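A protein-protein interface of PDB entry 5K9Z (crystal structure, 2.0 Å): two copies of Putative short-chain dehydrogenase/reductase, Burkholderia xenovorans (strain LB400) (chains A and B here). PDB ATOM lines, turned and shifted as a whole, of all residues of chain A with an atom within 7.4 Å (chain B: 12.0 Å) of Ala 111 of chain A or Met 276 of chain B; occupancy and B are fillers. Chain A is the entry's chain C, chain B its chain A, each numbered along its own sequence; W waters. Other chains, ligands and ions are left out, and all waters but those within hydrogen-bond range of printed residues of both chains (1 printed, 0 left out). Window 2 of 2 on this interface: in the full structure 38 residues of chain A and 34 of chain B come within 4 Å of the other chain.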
ATOM      1  N   PHE A  98      40.566  12.266   4.144  1.00  0.00           N
ATOM      2  CA  PHE A  98      39.236  11.814   4.535  1.00  0.00           C
ATOM      3  C   PHE A  98      38.457  11.469   3.275  1.00  0.00           C
ATOM      4  O   PHE A  98      38.548  12.192   2.282  1.00  0.00           O
ATOM      5  CB  PHE A  98      38.505  12.901   5.337  1.00  0.00           C
ATOM      6  CG  PHE A  98      37.121  12.508   5.779  1.00  0.00           C
ATOM      7  CD1 PHE A  98      36.925  11.809   6.960  1.00  0.00           C
ATOM      8  CD2 PHE A  98      36.013  12.832   5.010  1.00  0.00           C
ATOM      9  CE1 PHE A  98      35.636  11.455   7.383  1.00  0.00           C
ATOM     10  CE2 PHE A  98      34.729  12.466   5.419  1.00  0.00           C
ATOM     11  CZ  PHE A  98      34.541  11.780   6.597  1.00  0.00           C
ATOM     12  N   ALA A 101      31.616   8.542   2.792  1.00  0.00           N
ATOM     13  CA  ALA A 101      30.654   7.580   2.277  1.00  0.00           C
ATOM     14  C   ALA A 101      31.132   6.957   0.974  1.00  0.00           C
ATOM     15  O   ALA A 101      31.684   7.634   0.099  1.00  0.00           O
ATOM     16  CB  ALA A 101      29.306   8.262   2.060  1.00  0.00           C
ATOM     17  N   THR A 108      22.914   4.907   0.186  1.00  0.00           N
ATOM     18  CA  THR A 108      23.706   5.898   0.906  1.00  0.00           C
ATOM     19  C   THR A 108      22.789   6.727   1.795  1.00  0.00           C
ATOM     20  O   THR A 108      21.838   7.346   1.306  1.00  0.00           O
ATOM     21  CB  THR A 108      24.452   6.788  -0.082  1.00  0.00           C
ATOM     22  OG1 THR A 108      25.377   5.978  -0.814  1.00  0.00           O
ATOM     23  CG2 THR A 108      25.201   7.910   0.649  1.00  0.00           C
ATOM     24  N   SER A 109      23.067   6.741   3.094  1.00  0.00           N
ATOM     25  CA  SER A 109      22.207   7.461   4.018  1.00  0.00           C
ATOM     26  C   SER A 109      22.472   8.961   3.928  1.00  0.00           C
ATOM     27  O   SER A 109      23.560   9.397   3.544  1.00  0.00           O
ATOM     28  CB  SER A 109      22.442   6.984   5.447  1.00  0.00           C
ATOM     29  OG  SER A 109      23.716   7.400   5.910  1.00  0.00           O
ATOM     30  N   ALA A 110      21.452   9.748   4.288  1.00  0.00           N
ATOM     31  CA  ALA A 110      21.637  11.189   4.412  1.00  0.00           C
ATOM     32  C   ALA A 110      22.705  11.496   5.453  1.00  0.00           C
ATOM     33  O   ALA A 110      23.515  12.410   5.276  1.00  0.00           O
ATOM     34  CB  ALA A 110      20.302  11.858   4.774  1.00  0.00           C
ATOM     35  N   ALA A 111      22.749  10.715   6.532  1.00  0.00           N
ATOM     36  CA  ALA A 111      23.746  10.959   7.567  1.00  0.00           C
ATOM     37  C   ALA A 111      25.158  10.775   7.014  1.00  0.00           C
ATOM     38  O   ALA A 111      26.046  11.597   7.272  1.00  0.00           O
ATOM     39  CB  ALA A 111      23.490  10.036   8.770  1.00  0.00           C
ATOM     40  N   ALA A 112      25.382   9.712   6.237  1.00  0.00           N
ATOM     41  CA  ALA A 112      26.695   9.517   5.629  1.00  0.00           C
ATOM     42  C   ALA A 112      26.995  10.605   4.602  1.00  0.00           C
ATOM     43  O   ALA A 112      28.121  11.102   4.536  1.00  0.00           O
ATOM     44  CB  ALA A 112      26.785   8.134   4.988  1.00  0.00           C
ATOM     45  N   TRP A 113      25.991  10.986   3.802  1.00  0.00           N
ATOM     46  CA  TRP A 113      26.141  12.084   2.850  1.00  0.00           C
ATOM     47  C   TRP A 113      26.559  13.367   3.563  1.00  0.00           C
ATOM     48  O   TRP A 113      27.556  14.002   3.191  1.00  0.00           O
ATOM     49  CB  TRP A 113      24.817  12.253   2.081  1.00  0.00           C
ATOM     50  CG  TRP A 113      24.705  13.437   1.183  1.00  0.00           C
ATOM     51  CD1 TRP A 113      24.061  14.616   1.438  1.00  0.00           C
ATOM     52  CD2 TRP A 113      25.241  13.551  -0.143  1.00  0.00           C
ATOM     53  NE1 TRP A 113      24.173  15.458   0.350  1.00  0.00           N
ATOM     54  CE2 TRP A 113      24.893  14.825  -0.629  1.00  0.00           C
ATOM     55  CE3 TRP A 113      25.983  12.690  -0.967  1.00  0.00           C
ATOM     56  CZ2 TRP A 113      25.268  15.270  -1.899  1.00  0.00           C
ATOM     57  CZ3 TRP A 113      26.355  13.130  -2.232  1.00  0.00           C
ATOM     58  CH2 TRP A 113      26.005  14.415  -2.679  1.00  0.00           C
ATOM     59  N   HIS A 114      25.818  13.747   4.617  1.00  0.00           N
ATOM     60  CA  HIS A 114      26.097  14.991   5.332  1.00  0.00           C
ATOM     61  C   HIS A 114      27.427  14.950   6.076  1.00  0.00           C
ATOM     62  O   HIS A 114      28.141  15.958   6.115  1.00  0.00           O
ATOM     63  CB  HIS A 114      24.958  15.328   6.309  1.00  0.00           C
ATOM     64  CG  HIS A 114      23.710  15.793   5.627  1.00  0.00           C
ATOM     65  ND1 HIS A 114      22.477  15.228   5.863  1.00  0.00           N
ATOM     66  CD2 HIS A 114      23.521  16.710   4.649  1.00  0.00           C
ATOM     67  CE1 HIS A 114      21.571  15.814   5.101  1.00  0.00           C
ATOM     68  NE2 HIS A 114      22.181  16.710   4.346  1.00  0.00           N
ATOM     69  N   ALA A 115      27.760  13.819   6.713  1.00  0.00           N
ATOM     70  CA  ALA A 115      29.057  13.716   7.376  1.00  0.00           C
ATOM     71  C   ALA A 115      30.206  13.905   6.387  1.00  0.00           C
ATOM     72  O   ALA A 115      31.205  14.562   6.707  1.00  0.00           O
ATOM     73  CB  ALA A 115      29.198  12.366   8.082  1.00  0.00           C
ATOM     74  N   THR A 116      30.094  13.317   5.191  1.00  0.00           N
ATOM     75  CA  THR A 116      31.162  13.442   4.199  1.00  0.00           C
ATOM     76  C   THR A 116      31.318  14.892   3.757  1.00  0.00           C
ATOM     77  O   THR A 116      32.423  15.443   3.776  1.00  0.00           O
ATOM     78  CB  THR A 116      30.886  12.547   2.988  1.00  0.00           C
ATOM     79  OG1 THR A 116      30.772  11.183   3.406  1.00  0.00           O
ATOM     80  CG2 THR A 116      32.041  12.656   1.938  1.00  0.00           C
ATOM     81  N   LEU A 117      30.203  15.538   3.398  1.00  0.00           N
ATOM     82  CA  LEU A 117      30.248  16.921   2.923  1.00  0.00           C
ATOM     83  C   LEU A 117      30.652  17.896   4.028  1.00  0.00           C
ATOM     84  O   LEU A 117      31.233  18.946   3.735  1.00  0.00           O
ATOM     85  CB  LEU A 117      28.896  17.300   2.315  1.00  0.00           C
ATOM     86  CG  LEU A 117      28.720  17.062   0.799  1.00  0.00           C
ATOM     87  CD1 LEU A 117      29.108  15.670   0.363  1.00  0.00           C
ATOM     88  CD2 LEU A 117      27.275  17.328   0.414  1.00  0.00           C
ATOM     89  N   VAL A 119      33.034  17.539   6.225  1.00  0.00           N
ATOM     90  CA  VAL A 119      34.488  17.601   6.213  1.00  0.00           C
ATOM     91  C   VAL A 119      35.000  18.140   4.871  1.00  0.00           C
ATOM     92  O   VAL A 119      35.844  19.045   4.822  1.00  0.00           O
ATOM     93  CB  VAL A 119      35.081  16.207   6.512  1.00  0.00           C
ATOM     94  CG1 VAL A 119      36.583  16.247   6.430  1.00  0.00           C
ATOM     95  CG2 VAL A 119      34.594  15.644   7.893  1.00  0.00           C
ATOM     96  N   ALA B 270      26.715  -0.069   0.629  1.00  0.00           N
ATOM     97  CA  ALA B 270      26.949   1.292   1.102  1.00  0.00           C
ATOM     98  C   ALA B 270      27.645   1.259   2.455  1.00  0.00           C
ATOM     99  O   ALA B 270      27.235   0.529   3.368  1.00  0.00           O
ATOM    100  CB  ALA B 270      25.635   2.061   1.189  1.00  0.00           C
ATOM    101  N   GLY B 271      28.722   2.024   2.569  1.00  0.00           N
ATOM    102  CA  GLY B 271      29.488   2.037   3.797  1.00  0.00           C
ATOM    103  C   GLY B 271      30.086   3.395   4.079  1.00  0.00           C
ATOM    104  O   GLY B 271      29.790   4.365   3.380  1.00  0.00           O
ATOM    105  N   PHE B 272      30.931   3.486   5.099  1.00  0.00           N
ATOM    106  CA  PHE B 272      31.494   4.776   5.461  1.00  0.00           C
ATOM    107  C   PHE B 272      32.913   4.554   5.955  1.00  0.00           C
ATOM    108  O   PHE B 272      33.135   3.755   6.867  1.00  0.00           O
ATOM    109  CB  PHE B 272      30.620   5.462   6.526  1.00  0.00           C
ATOM    110  CG  PHE B 272      31.010   6.888   6.808  1.00  0.00           C
ATOM    111  CD1 PHE B 272      32.023   7.184   7.707  1.00  0.00           C
ATOM    112  CD2 PHE B 272      30.358   7.934   6.170  1.00  0.00           C
ATOM    113  CE1 PHE B 272      32.381   8.502   7.965  1.00  0.00           C
ATOM    114  CE2 PHE B 272      30.701   9.253   6.425  1.00  0.00           C
ATOM    115  CZ  PHE B 272      31.719   9.538   7.321  1.00  0.00           C
ATOM    116  N   MET B 273      33.868   5.238   5.338  1.00  0.00           N
ATOM    117  CA  MET B 273      35.264   5.200   5.755  1.00  0.00           C
ATOM    118  C   MET B 273      35.572   6.442   6.582  1.00  0.00           C
ATOM    119  O   MET B 273      35.546   7.560   6.055  1.00  0.00           O
ATOM    120  CB  MET B 273      36.193   5.150   4.544  1.00  0.00           C
ATOM    121  CG  MET B 273      36.070   3.930   3.671  1.00  0.00           C
ATOM    122  SD  MET B 273      37.282   4.029   2.330  1.00  0.00           S
ATOM    123  CE  MET B 273      36.235   4.365   0.918  1.00  0.00           C
ATOM    124  N   GLY B 274      35.879   6.252   7.855  1.00  0.00           N
ATOM    125  CA  GLY B 274      36.308   7.336   8.718  1.00  0.00           C
ATOM    126  C   GLY B 274      35.353   7.555   9.876  1.00  0.00           C
ATOM    127  O   GLY B 274      34.454   6.751  10.145  1.00  0.00           O
ATOM    128  N   ARG B 275      35.567   8.671  10.576  1.00  0.00           N
ATOM    129  CA  ARG B 275      34.790   9.034  11.756  1.00  0.00           C
ATOM    130  C   ARG B 275      33.517   9.777  11.360  1.00  0.00           C
ATOM    131  O   ARG B 275      33.575  10.778  10.635  1.00  0.00           O
ATOM    132  CB  ARG B 275      35.634   9.896  12.694  1.00  0.00           C
ATOM    133  N   MET B 276      32.375   9.304  11.854  1.00  0.00           N
ATOM    134  CA  MET B 276      31.085   9.927  11.547  1.00  0.00           C
ATOM    135  C   MET B 276      30.967  11.336  12.137  1.00  0.00           C
ATOM    136  O   MET B 276      30.219  11.572  13.086  1.00  0.00           O
ATOM    137  CB  MET B 276      29.933   9.046  12.045  1.00  0.00           C
ATOM    138  CG  MET B 276      29.437   8.035  11.011  1.00  0.00           C
ATOM    139  SD  MET B 276      28.601   8.843   9.622  1.00  0.00           S
ATOM    140  CE  MET B 276      27.050   9.304  10.399  1.00  0.00           C
HETATM  141  O   HOH W   1      27.327   5.167   1.905  1.00  0.00           O
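Among the printed residues, pairs that only touch across the chains: Phe 98 of chain A with Phe 272 of chain B (3.7 Å), Phe 98 of chain A with Arg 275 of chain B (3.9 Å), Ala 101 of chain A with Gly 271 of chain B (3.5 Å), Ala 101 of chain A with Phe 272 of chain B (3.7 Å), Ala 111 of chain A with Met 276 of chain B (3.98 Å), Ala 112 of chain A with Phe 272 of chain B (3.7 Å), Ala 115 of chain A with Phe 272 of chain B (3.8 Å), Ala 115 of chain A with Met 276 of chain B (3.9 Å) and Thr 116 of chain A with Phe 272 of chain B (3.6 Å).
No position is printed for both chains.
Of the 9 pairs that touch across the chains among the printed residues, none has its exchanged pair printed and touching as well.
Printed residues of chain B within 4 Å of Ala 101 of chain A: Gly 271 and Phe 272.
Of the printed residues of chain B, Ala 111 of chain A touches Met 276 (3.98 Å).
Printed residues of chain B within 4 Å of Ala 112 of chain A: Phe 272.
Leu 117 of chain A touches none of the printed residues of chain B.
Printed residues of chain A within 4 Å of Gly 271 of chain B: Ala 101.
Of the printed residues of chain A, Met 276 of chain B touches Ala 111 and Ala 115.
The nearest printed residue of chain B that does not touch Ala 111 of chain A is Phe 272 of chain B (5.3 Å).
The nearest printed residue of chain A that does not touch Met 276 of chain B is Ala 112 of chain A (4.5 Å).
The nearest printed residue of chain B that does not touch Ala 101 of chain A is Met 273 of chain B (4.7 Å).
The side-chain hydroxyl (OG) of Ser 109 of chain A lies within hydrogen-bond range of the backbone NH (N) of Ala 112 of chain A (2.9 Å).
The backbone carbonyl oxygen (O) of Ala 112 of chain A sits at hydrogen-bond distance from the side-chain hydroxyl (OG1) of Thr 116 of chain A, at 2.9 Å.
The side-chain hydroxyl (OG1) of Thr 116 of chain A lies within hydrogen-bond range of the backbone NH (N) of Ala 101 of chain A (2.8 Å).
Water W1 lies within hydrogen-bond range of O of Gly 271 of chain B (3.0 Å) and OG1 of Thr 108 of chain A (3.4 Å).
Printed residues of chain A that touch a printed residue of chain B: Phe 98, Ala 101, Ala 111, Ala 112, Ala 115 and Thr 116.
Printed residues of chain B that touch a printed residue of chain A: Gly 271, Phe 272, Arg 275 and Met 276.
Hydrophobic or aromatic side chains of chain B within 4 Å of the printed part of chain A: Phe 272 and Met 276.
Among the printed residues, no Asp or Glu carboxylate lies within 4 Å of a Lys or Arg side-chain nitrogen of the other chain.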
